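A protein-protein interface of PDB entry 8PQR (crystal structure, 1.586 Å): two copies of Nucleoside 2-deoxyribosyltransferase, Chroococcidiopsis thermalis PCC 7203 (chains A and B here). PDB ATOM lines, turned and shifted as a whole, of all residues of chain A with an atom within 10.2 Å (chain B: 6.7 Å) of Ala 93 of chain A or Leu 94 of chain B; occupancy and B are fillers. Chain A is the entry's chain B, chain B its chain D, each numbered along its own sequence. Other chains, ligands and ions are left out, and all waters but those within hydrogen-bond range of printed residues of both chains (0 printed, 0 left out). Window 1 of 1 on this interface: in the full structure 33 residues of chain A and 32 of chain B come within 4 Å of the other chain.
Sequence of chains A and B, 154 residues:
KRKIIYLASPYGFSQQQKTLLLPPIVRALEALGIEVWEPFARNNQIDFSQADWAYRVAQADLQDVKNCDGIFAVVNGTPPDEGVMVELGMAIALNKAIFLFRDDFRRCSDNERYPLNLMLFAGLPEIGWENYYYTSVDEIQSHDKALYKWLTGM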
ATOM      1  N   LEU A  62       4.643  24.536 -15.266  1.00  0.00           N
ATOM      2  CA  LEU A  62       5.756  24.021 -16.059  1.00  0.00           C
ATOM      3  C   LEU A  62       5.782  22.498 -16.041  1.00  0.00           C
ATOM      4  O   LEU A  62       5.926  21.851 -17.089  1.00  0.00           O
ATOM      5  CB  LEU A  62       7.073  24.581 -15.517  1.00  0.00           C
ATOM      6  CG  LEU A  62       8.396  24.320 -16.237  1.00  0.00           C
ATOM      7  CD1 LEU A  62       9.324  25.512 -16.053  1.00  0.00           C
ATOM      8  CD2 LEU A  62       9.065  23.059 -15.727  1.00  0.00           C
ATOM      9  N   VAL A  65       2.816  21.001 -18.122  1.00  0.00           N
ATOM     10  CA  VAL A  65       3.004  21.010 -19.571  1.00  0.00           C
ATOM     11  C   VAL A  65       4.013  19.940 -19.976  1.00  0.00           C
ATOM     12  O   VAL A  65       3.850  19.260 -20.998  1.00  0.00           O
ATOM     13  CB  VAL A  65       3.436  22.406 -20.054  1.00  0.00           C
ATOM     14  CG1 VAL A  65       3.805  22.371 -21.543  1.00  0.00           C
ATOM     15  CG2 VAL A  65       2.330  23.432 -19.791  1.00  0.00           C
ATOM     16  N   LYS A  66       5.054  19.745 -19.161  1.00  0.00           N
ATOM     17  CA  LYS A  66       6.020  18.686 -19.437  1.00  0.00           C
ATOM     18  C   LYS A  66       5.379  17.307 -19.381  1.00  0.00           C
ATOM     19  O   LYS A  66       5.784  16.406 -20.120  1.00  0.00           O
ATOM     20  CB  LYS A  66       7.184  18.755 -18.445  1.00  0.00           C
ATOM     21  CG  LYS A  66       8.143  19.914 -18.669  1.00  0.00           C
ATOM     22  CD  LYS A  66       9.203  19.940 -17.576  1.00  0.00           C
ATOM     23  CE  LYS A  66      10.471  20.655 -18.023  1.00  0.00           C
ATOM     24  NZ  LYS A  66      11.384  20.943 -16.875  1.00  0.00           N
ATOM     25  N   ILE A  71      -1.685  19.963 -25.464  1.00  0.00           N
ATOM     26  CA  ILE A  71      -2.210  21.219 -24.946  1.00  0.00           C
ATOM     27  C   ILE A  71      -3.420  21.610 -25.778  1.00  0.00           C
ATOM     28  O   ILE A  71      -3.420  21.463 -27.006  1.00  0.00           O
ATOM     29  CB  ILE A  71      -1.149  22.338 -24.941  1.00  0.00           C
ATOM     30  CG1 ILE A  71      -1.698  23.579 -24.221  1.00  0.00           C
ATOM     31  CG2 ILE A  71      -0.704  22.679 -26.350  1.00  0.00           C
ATOM     32  CD1 ILE A  71      -0.663  24.669 -23.998  1.00  0.00           C
ATOM     33  N   MET A  85       0.552  31.698 -24.069  1.00  0.00           N
ATOM     34  CA  MET A  85       1.552  31.649 -25.136  1.00  0.00           C
ATOM     35  C   MET A  85       2.854  31.016 -24.662  1.00  0.00           C
ATOM     36  O   MET A  85       3.470  30.247 -25.403  1.00  0.00           O
ATOM     37  CB  MET A  85       1.811  33.054 -25.669  1.00  0.00           C
ATOM     38  CG  MET A  85       0.604  33.699 -26.366  1.00  0.00           C
ATOM     39  SD  MET A  85       0.164  32.791 -27.864  1.00  0.00           S
ATOM     40  CE  MET A  85      -1.143  31.693 -27.307  1.00  0.00           C
ATOM     41  N   VAL A  86       3.294  31.327 -23.440  1.00  0.00           N
ATOM     42  CA  VAL A  86       4.485  30.667 -22.894  1.00  0.00           C
ATOM     43  C   VAL A  86       4.256  29.162 -22.812  1.00  0.00           C
ATOM     44  O   VAL A  86       5.118  28.360 -23.195  1.00  0.00           O
ATOM     45  CB  VAL A  86       4.851  31.254 -21.519  1.00  0.00           C
ATOM     46  CG1 VAL A  86       5.969  30.437 -20.882  1.00  0.00           C
ATOM     47  CG2 VAL A  86       5.293  32.709 -21.652  1.00  0.00           C
ATOM     48  N   GLU A  87       3.089  28.755 -22.309  1.00  0.00           N
ATOM     49  CA  GLU A  87       2.798  27.323 -22.202  1.00  0.00           C
ATOM     50  C   GLU A  87       2.724  26.671 -23.580  1.00  0.00           C
ATOM     51  O   GLU A  87       3.146  25.520 -23.756  1.00  0.00           O
ATOM     52  CB  GLU A  87       1.495  27.123 -21.420  1.00  0.00           C
ATOM     53  CG  GLU A  87       1.627  27.599 -19.980  1.00  0.00           C
ATOM     54  CD  GLU A  87       0.295  27.899 -19.303  1.00  0.00           C
ATOM     55  OE1 GLU A  87      -0.744  28.006 -19.997  1.00  0.00           O
ATOM     56  OE2 GLU A  87       0.298  28.031 -18.059  1.00  0.00           O
ATOM     57  N   LEU A  88       2.176  27.389 -24.565  1.00  0.00           N
ATOM     58  CA  LEU A  88       2.140  26.879 -25.935  1.00  0.00           C
ATOM     59  C   LEU A  88       3.546  26.698 -26.502  1.00  0.00           C
ATOM     60  O   LEU A  88       3.843  25.673 -27.132  1.00  0.00           O
ATOM     61  CB  LEU A  88       1.311  27.828 -26.813  1.00  0.00           C
ATOM     62  CG  LEU A  88       1.283  27.550 -28.315  1.00  0.00           C
ATOM     63  CD1 LEU A  88       0.692  26.171 -28.581  1.00  0.00           C
ATOM     64  CD2 LEU A  88       0.469  28.617 -29.020  1.00  0.00           C
ATOM     65  N   GLY A  89       4.426  27.679 -26.283  1.00  0.00           N
ATOM     66  CA  GLY A  89       5.800  27.544 -26.739  1.00  0.00           C
ATOM     67  C   GLY A  89       6.497  26.361 -26.092  1.00  0.00           C
ATOM     68  O   GLY A  89       7.236  25.632 -26.754  1.00  0.00           O
ATOM     69  N   MET A  90       6.262  26.154 -24.789  1.00  0.00           N
ATOM     70  CA  MET A  90       6.785  24.962 -24.127  1.00  0.00           C
ATOM     71  C   MET A  90       6.278  23.694 -24.806  1.00  0.00           C
ATOM     72  O   MET A  90       7.060  22.790 -25.124  1.00  0.00           O
ATOM     73  CB  MET A  90       6.404  24.959 -22.641  1.00  0.00           C
ATOM     74  CG  MET A  90       7.033  26.094 -21.858  1.00  0.00           C
ATOM     75  SD  MET A  90       6.433  26.139 -20.154  1.00  0.00           S
ATOM     76  CE  MET A  90       6.996  24.532 -19.579  1.00  0.00           C
ATOM     77  N   ALA A  91       4.969  23.623 -25.061  1.00  0.00           N
ATOM     78  CA  ALA A  91       4.390  22.431 -25.676  1.00  0.00           C
ATOM     79  C   ALA A  91       4.984  22.159 -27.054  1.00  0.00           C
ATOM     80  O   ALA A  91       5.262  21.004 -27.396  1.00  0.00           O
ATOM     81  CB  ALA A  91       2.868  22.576 -25.767  1.00  0.00           C
ATOM     82  N   ILE A  92       5.162  23.204 -27.868  1.00  0.00           N
ATOM     83  CA  ILE A  92       5.767  23.026 -29.188  1.00  0.00           C
ATOM     84  C   ILE A  92       7.177  22.459 -29.050  1.00  0.00           C
ATOM     85  O   ILE A  92       7.539  21.469 -29.699  1.00  0.00           O
ATOM     86  CB  ILE A  92       5.765  24.358 -29.964  1.00  0.00           C
ATOM     87  CG1 ILE A  92       4.338  24.841 -30.207  1.00  0.00           C
ATOM     88  CG2 ILE A  92       6.514  24.222 -31.304  1.00  0.00           C
ATOM     89  CD1 ILE A  92       4.268  26.306 -30.681  1.00  0.00           C
ATOM     90  N   ALA A  93       7.984  23.066 -28.175  1.00  0.00           N
ATOM     91  CA  ALA A  93       9.375  22.638 -28.030  1.00  0.00           C
ATOM     92  C   ALA A  93       9.480  21.220 -27.477  1.00  0.00           C
ATOM     93  O   ALA A  93      10.450  20.509 -27.779  1.00  0.00           O
ATOM     94  CB  ALA A  93      10.135  23.620 -27.132  1.00  0.00           C
ATOM     95  N   LEU A  94       8.497  20.791 -26.684  1.00  0.00           N
ATOM     96  CA  LEU A  94       8.500  19.476 -26.060  1.00  0.00           C
ATOM     97  C   LEU A  94       7.761  18.430 -26.882  1.00  0.00           C
ATOM     98  O   LEU A  94       7.576  17.305 -26.411  1.00  0.00           O
ATOM     99  CB  LEU A  94       7.905  19.563 -24.664  1.00  0.00           C
ATOM    100  CG  LEU A  94       8.714  20.392 -23.686  1.00  0.00           C
ATOM    101  CD1 LEU A  94       7.959  20.555 -22.363  1.00  0.00           C
ATOM    102  CD2 LEU A  94      10.065  19.744 -23.492  1.00  0.00           C
ATOM    103  N   ASN A  95       7.400  18.761 -28.126  1.00  0.00           N
ATOM    104  CA  ASN A  95       6.752  17.856 -29.089  1.00  0.00           C
ATOM    105  C   ASN A  95       5.430  17.321 -28.573  1.00  0.00           C
ATOM    106  O   ASN A  95       5.044  16.188 -28.878  1.00  0.00           O
ATOM    107  CB  ASN A  95       7.658  16.692 -29.477  1.00  0.00           C
ATOM    108  CG  ASN A  95       8.887  17.143 -30.158  1.00  0.00           C
ATOM    109  OD1 ASN A  95       9.996  16.900 -29.664  1.00  0.00           O
ATOM    110  ND2 ASN A  95       8.729  17.748 -31.334  1.00  0.00           N
ATOM    111  N   LYS A  96       4.731  18.128 -27.784  1.00  0.00           N
ATOM    112  CA  LYS A  96       3.385  17.751 -27.392  1.00  0.00           C
ATOM    113  C   LYS A  96       2.392  17.953 -28.542  1.00  0.00           C
ATOM    114  O   LYS A  96       2.603  18.754 -29.459  1.00  0.00           O
ATOM    115  CB  LYS A  96       2.936  18.578 -26.181  1.00  0.00           C
ATOM    116  CG  LYS A  96       3.894  18.488 -25.004  1.00  0.00           C
ATOM    117  CD  LYS A  96       3.982  17.064 -24.492  1.00  0.00           C
ATOM    118  CE  LYS A  96       4.949  16.941 -23.327  1.00  0.00           C
ATOM    119  NZ  LYS A  96       4.951  15.560 -22.768  1.00  0.00           N
ATOM    120  N   ALA A  97       1.271  17.238 -28.464  1.00  0.00           N
ATOM    121  CA  ALA A  97       0.168  17.536 -29.371  1.00  0.00           C
ATOM    122  C   ALA A  97      -0.373  18.934 -29.103  1.00  0.00           C
ATOM    123  O   ALA A  97      -0.442  19.385 -27.955  1.00  0.00           O
ATOM    124  CB  ALA A  97      -0.949  16.511 -29.222  1.00  0.00           C
ATOM    125  N   ILE A  98      -0.752  19.625 -30.177  1.00  0.00           N
ATOM    126  CA  ILE A  98      -1.159  21.026 -30.117  1.00  0.00           C
ATOM    127  C   ILE A  98      -2.557  21.168 -30.703  1.00  0.00           C
ATOM    128  O   ILE A  98      -2.783  20.810 -31.865  1.00  0.00           O
ATOM    129  CB  ILE A  98      -0.186  21.938 -30.878  1.00  0.00           C
ATOM    130  CG1 ILE A  98       1.260  21.693 -30.453  1.00  0.00           C
ATOM    131  CG2 ILE A  98      -0.584  23.406 -30.685  1.00  0.00           C
ATOM    132  CD1 ILE A  98       1.610  22.284 -29.132  1.00  0.00           C
ATOM    133  N   MET A 119       3.686  32.616 -35.108  1.00  0.00           N
ATOM    134  CA  MET A 119       4.400  31.734 -34.177  1.00  0.00           C
ATOM    135  C   MET A 119       3.472  30.727 -33.511  1.00  0.00           C
ATOM    136  O   MET A 119       3.923  29.654 -33.088  1.00  0.00           O
ATOM    137  CB  MET A 119       5.102  32.540 -33.087  1.00  0.00           C
ATOM    138  CG  MET A 119       6.391  33.191 -33.511  1.00  0.00           C
ATOM    139  SD  MET A 119       7.541  32.082 -34.351  1.00  0.00           S
ATOM    140  CE  MET A 119       7.741  30.754 -33.168  1.00  0.00           C
ATOM    141  N   LEU A 120       2.192  31.070 -33.355  1.00  0.00           N
ATOM    142  CA  LEU A 120       1.265  30.174 -32.663  1.00  0.00           C
ATOM    143  C   LEU A 120       1.052  28.873 -33.419  1.00  0.00           C
ATOM    144  O   LEU A 120       0.547  27.904 -32.838  1.00  0.00           O
ATOM    145  CB  LEU A 120      -0.077  30.864 -32.444  1.00  0.00           C
ATOM    146  CG  LEU A 120      -0.168  31.785 -31.227  1.00  0.00           C
ATOM    147  CD1 LEU A 120       0.649  33.071 -31.472  1.00  0.00           C
ATOM    148  CD2 LEU A 120      -1.617  32.115 -30.952  1.00  0.00           C
ATOM    149  N   ALA A 122       3.546  27.246 -35.168  1.00  0.00           N
ATOM    150  CA  ALA A 122       4.845  26.659 -35.486  1.00  0.00           C
ATOM    151  C   ALA A 122       4.889  25.157 -35.217  1.00  0.00           C
ATOM    152  O   ALA A 122       5.692  24.448 -35.829  1.00  0.00           O
ATOM    153  CB  ALA A 122       5.945  27.378 -34.704  1.00  0.00           C
ATOM    154  N   GLY A 123       4.055  24.657 -34.308  1.00  0.00           N
ATOM    155  CA  GLY A 123       3.961  23.242 -34.024  1.00  0.00           C
ATOM    156  C   GLY A 123       2.877  22.514 -34.778  1.00  0.00           C
ATOM    157  O   GLY A 123       2.644  21.330 -34.522  1.00  0.00           O
ATOM    158  N   LEU A 124       2.181  23.192 -35.683  1.00  0.00           N
ATOM    159  CA  LEU A 124       1.137  22.605 -36.508  1.00  0.00           C
ATOM    160  C   LEU A 124       1.644  22.384 -37.925  1.00  0.00           C
ATOM    161  O   LEU A 124       2.612  23.021 -38.358  1.00  0.00           O
ATOM    162  CB  LEU A 124      -0.100  23.510 -36.521  1.00  0.00           C
ATOM    163  CG  LEU A 124      -0.819  23.587 -35.176  1.00  0.00           C
ATOM    164  CD1 LEU A 124      -2.044  24.501 -35.248  1.00  0.00           C
ATOM    165  CD2 LEU A 124      -1.205  22.186 -34.723  1.00  0.00           C
ATOM    166  N   LEU B  62      11.729  29.074 -34.944  1.00  0.00           N
ATOM    167  CA  LEU B  62      11.810  27.893 -34.093  1.00  0.00           C
ATOM    168  C   LEU B  62      13.228  27.327 -34.077  1.00  0.00           C
ATOM    169  O   LEU B  62      13.782  27.019 -33.013  1.00  0.00           O
ATOM    170  CB  LEU B  62      10.803  26.855 -34.595  1.00  0.00           C
ATOM    171  CG  LEU B  62      10.417  25.591 -33.830  1.00  0.00           C
ATOM    172  CD1 LEU B  62       8.957  25.281 -34.119  1.00  0.00           C
ATOM    173  CD2 LEU B  62      11.282  24.430 -34.248  1.00  0.00           C
ATOM    174  N   VAL B  65      15.702  29.540 -32.085  1.00  0.00           N
ATOM    175  CA  VAL B  65      15.600  29.360 -30.640  1.00  0.00           C
ATOM    176  C   VAL B  65      16.256  28.052 -30.228  1.00  0.00           C
ATOM    177  O   VAL B  65      16.958  27.985 -29.209  1.00  0.00           O
ATOM    178  CB  VAL B  65      14.129  29.424 -30.183  1.00  0.00           C
ATOM    179  CG1 VAL B  65      14.044  29.245 -28.675  1.00  0.00           C
ATOM    180  CG2 VAL B  65      13.507  30.737 -30.571  1.00  0.00           C
ATOM    181  N   LYS B  66      16.065  26.994 -31.027  1.00  0.00           N
ATOM    182  CA  LYS B  66      16.689  25.711 -30.719  1.00  0.00           C
ATOM    183  C   LYS B  66      18.209  25.805 -30.724  1.00  0.00           C
ATOM    184  O   LYS B  66      18.878  25.114 -29.949  1.00  0.00           O
ATOM    185  CB  LYS B  66      16.213  24.648 -31.710  1.00  0.00           C
ATOM    186  CG  LYS B  66      14.760  24.202 -31.483  1.00  0.00           C
ATOM    187  CD  LYS B  66      14.272  23.312 -32.620  1.00  0.00           C
ATOM    188  CE  LYS B  66      13.920  21.911 -32.147  1.00  0.00           C
ATOM    189  NZ  LYS B  66      13.817  20.962 -33.291  1.00  0.00           N
ATOM    190  N   ASN B  67      18.770  26.672 -31.562  1.00  0.00           N
ATOM    191  CA  ASN B  67      20.211  26.747 -31.766  1.00  0.00           C
ATOM    192  C   ASN B  67      20.878  27.914 -31.046  1.00  0.00           C
ATOM    193  O   ASN B  67      22.109  28.031 -31.101  1.00  0.00           O
ATOM    194  CB  ASN B  67      20.515  26.827 -33.264  1.00  0.00           C
ATOM    195  CG  ASN B  67      20.190  25.539 -33.983  1.00  0.00           C
ATOM    196  OD1 ASN B  67      20.302  24.457 -33.411  1.00  0.00           O
ATOM    197  ND2 ASN B  67      19.791  25.644 -35.243  1.00  0.00           N
ATOM    198  N   GLY B  89       8.629  30.607 -24.206  1.00  0.00           N
ATOM    199  CA  GLY B  89       8.263  29.274 -23.746  1.00  0.00           C
ATOM    200  C   GLY B  89       9.123  28.191 -24.371  1.00  0.00           C
ATOM    201  O   GLY B  89       9.534  27.242 -23.697  1.00  0.00           O
ATOM    202  N   MET B  90       9.419  28.324 -25.667  1.00  0.00           N
ATOM    203  CA  MET B  90      10.341  27.395 -26.303  1.00  0.00           C
ATOM    204  C   MET B  90      11.689  27.406 -25.596  1.00  0.00           C
ATOM    205  O   MET B  90      12.262  26.348 -25.305  1.00  0.00           O
ATOM    206  CB  MET B  90      10.513  27.751 -27.779  1.00  0.00           C
ATOM    207  CG  MET B  90       9.301  27.456 -28.608  1.00  0.00           C
ATOM    208  SD  MET B  90       9.428  28.285 -30.196  1.00  0.00           S
ATOM    209  CE  MET B  90       7.982  27.642 -31.040  1.00  0.00           C
ATOM    210  N   ALA B  91      12.207  28.603 -25.305  1.00  0.00           N
ATOM    211  CA  ALA B  91      13.525  28.717 -24.686  1.00  0.00           C
ATOM    212  C   ALA B  91      13.536  28.105 -23.289  1.00  0.00           C
ATOM    213  O   ALA B  91      14.514  27.456 -22.891  1.00  0.00           O
ATOM    214  CB  ALA B  91      13.942  30.187 -24.628  1.00  0.00           C
ATOM    215  N   ILE B  92      12.463  28.306 -22.526  1.00  0.00           N
ATOM    216  CA  ILE B  92      12.371  27.681 -21.206  1.00  0.00           C
ATOM    217  C   ILE B  92      12.401  26.159 -21.341  1.00  0.00           C
ATOM    218  O   ILE B  92      13.188  25.469 -20.675  1.00  0.00           O
ATOM    219  CB  ILE B  92      11.104  28.162 -20.471  1.00  0.00           C
ATOM    220  CG1 ILE B  92      11.194  29.656 -20.156  1.00  0.00           C
ATOM    221  CG2 ILE B  92      10.883  27.357 -19.182  1.00  0.00           C
ATOM    222  CD1 ILE B  92       9.835  30.311 -19.854  1.00  0.00           C
ATOM    223  N   ALA B  93      11.552  25.619 -22.219  1.00  0.00           N
ATOM    224  CA  ALA B  93      11.455  24.170 -22.385  1.00  0.00           C
ATOM    225  C   ALA B  93      12.745  23.568 -22.913  1.00  0.00           C
ATOM    226  O   ALA B  93      13.014  22.380 -22.675  1.00  0.00           O
ATOM    227  CB  ALA B  93      10.306  23.826 -23.330  1.00  0.00           C
ATOM    228  N   LEU B  94      13.541  24.350 -23.645  1.00  0.00           N
ATOM    229  CA  LEU B  94      14.793  23.867 -24.221  1.00  0.00           C
ATOM    230  C   LEU B  94      15.996  24.164 -23.338  1.00  0.00           C
ATOM    231  O   LEU B  94      17.136  23.971 -23.774  1.00  0.00           O
ATOM    232  CB  LEU B  94      14.999  24.467 -25.612  1.00  0.00           C
ATOM    233  CG  LEU B  94      13.928  24.069 -26.623  1.00  0.00           C
ATOM    234  CD1 LEU B  94      13.993  24.947 -27.861  1.00  0.00           C
ATOM    235  CD2 LEU B  94      14.072  22.595 -26.984  1.00  0.00           C
ATOM    236  N   ASN B  95      15.765  24.650 -22.117  1.00  0.00           N
ATOM    237  CA  ASN B  95      16.814  24.878 -21.129  1.00  0.00           C
ATOM    238  C   ASN B  95      17.829  25.919 -21.584  1.00  0.00           C
ATOM    239  O   ASN B  95      19.014  25.838 -21.232  1.00  0.00           O
ATOM    240  CB  ASN B  95      17.513  23.563 -20.767  1.00  0.00           C
ATOM    241  CG  ASN B  95      16.528  22.511 -20.312  1.00  0.00           C
ATOM    242  OD1 ASN B  95      16.327  21.487 -20.971  1.00  0.00           O
ATOM    243  ND2 ASN B  95      15.876  22.782 -19.200  1.00  0.00           N
ATOM    244  N   LYS B  96      17.382  26.900 -22.365  1.00  0.00           N
ATOM    245  CA  LYS B  96      18.243  28.002 -22.757  1.00  0.00           C
ATOM    246  C   LYS B  96      18.355  29.024 -21.626  1.00  0.00           C
ATOM    247  O   LYS B  96      17.493  29.113 -20.749  1.00  0.00           O
ATOM    248  CB  LYS B  96      17.706  28.676 -24.030  1.00  0.00           C
ATOM    249  CG  LYS B  96      17.458  27.706 -25.192  1.00  0.00           C
ATOM    250  CD  LYS B  96      18.761  27.080 -25.676  1.00  0.00           C
ATOM    251  CE  LYS B  96      18.564  26.150 -26.877  1.00  0.00           C
ATOM    252  NZ  LYS B  96      19.861  25.654 -27.420  1.00  0.00           N
ATOM    253  N   ALA B  97      19.431  29.811 -21.658  1.00  0.00           N
ATOM    254  CA  ALA B  97      19.517  30.950 -20.748  1.00  0.00           C
ATOM    255  C   ALA B  97      18.395  31.940 -21.041  1.00  0.00           C
ATOM    256  O   ALA B  97      18.017  32.147 -22.198  1.00  0.00           O
ATOM    257  CB  ALA B  97      20.881  31.631 -20.874  1.00  0.00           C
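Ile 92 of chain B touches Leu 62 of chain A (CG2 to CD1, 3.95 Å).
Val 86 of chain A touches Gly 89 of chain B (O to CA, 3.3 Å).
Met 90 of chain B touches Gly 89 of chain A (CG to O, 3.3 Å).
O of Gly 89 of chain B touches CG of Met 90 of chain A (3.3 Å).
Met 90 of chain A touches Ala 93 of chain B (CA to CB, 3.8 Å).
CG2 of Ile 92 of chain A touches CE of Met 90 of chain B, at 3.7 Å.
CB of Ala 93 of chain A touches CB of Ala 93 of chain B, 3.8 Å away.
Leu 94 of chain A touches Ala 93 of chain B.
CE of Met 90 of chain B touches CE of Met 119 of chain A, at 3.8 Å.
Ala 122 of chain A touches Leu 62 of chain B (CB to CD1, 3.7 Å).
Leu 62 of chain A touches Ile 92 of chain B, and with the chains exchanged Ile 92 of chain A touches Leu 62 of chain B.
Ile 92 of chain A touches Met 90 of chain B, but with the chains exchanged Met 90 of chain A does not touch Ile 92 of chain B (4.7 Å).
Ala 93 of chain B touches its own counterpart, Ala 93 of chain A.
Ala 93 of chain A touches Leu 94 of chain B, and with the chains exchanged Leu 94 of chain A touches Ala 93 of chain B.
Positions printed for both chains: 62, 65, 66, 89, 90, 91, 92, 93, 94, 95, 96 and 97.
Of the printed residues of chain B, Val 86 of chain A touches Gly 89 (3.3 Å).
Leu 88 of chain A touches none of the printed residues of chain B.
Of the printed residues of chain B, Gly 89 of chain A touches Gly 89 and Met 90.
Ala 93 of chain A touches just these residues of chain B: Met 90 (3.9 Å), Ala 93 (3.8 Å) and Leu 94 (3.9 Å).
Lys 96 of chain A touches none of the printed residues of chain B.
Printed residues of chain B within 4 Å of Ala 122 of chain A: Leu 62 (3.7 Å).
Of the printed residues of chain A, Leu 62 of chain B touches Ile 92 (3.9 Å) and Ala 122 (3.7 Å).
Met 90 of chain B touches five residues of chain A.
Of chain A, only Ala 93 comes within 4 Å of Leu 94 of chain B.
No residue of chain A comes within 4 Å of Asn 95 of chain B.
No residue of chain A comes within 4 Å of Lys 96 of chain B.
The nearest residue of chain B that does not touch Ala 93 of chain A is Gly 89 of chain B (5.0 Å).
Of the 13 printed residues of chain B, 6 touch a printed residue of chain A.
Along chain B the printed residues that touch a printed residue of chain A span positions 62 to 94.
Among the printed residues, 15 pairs touch across the chains.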
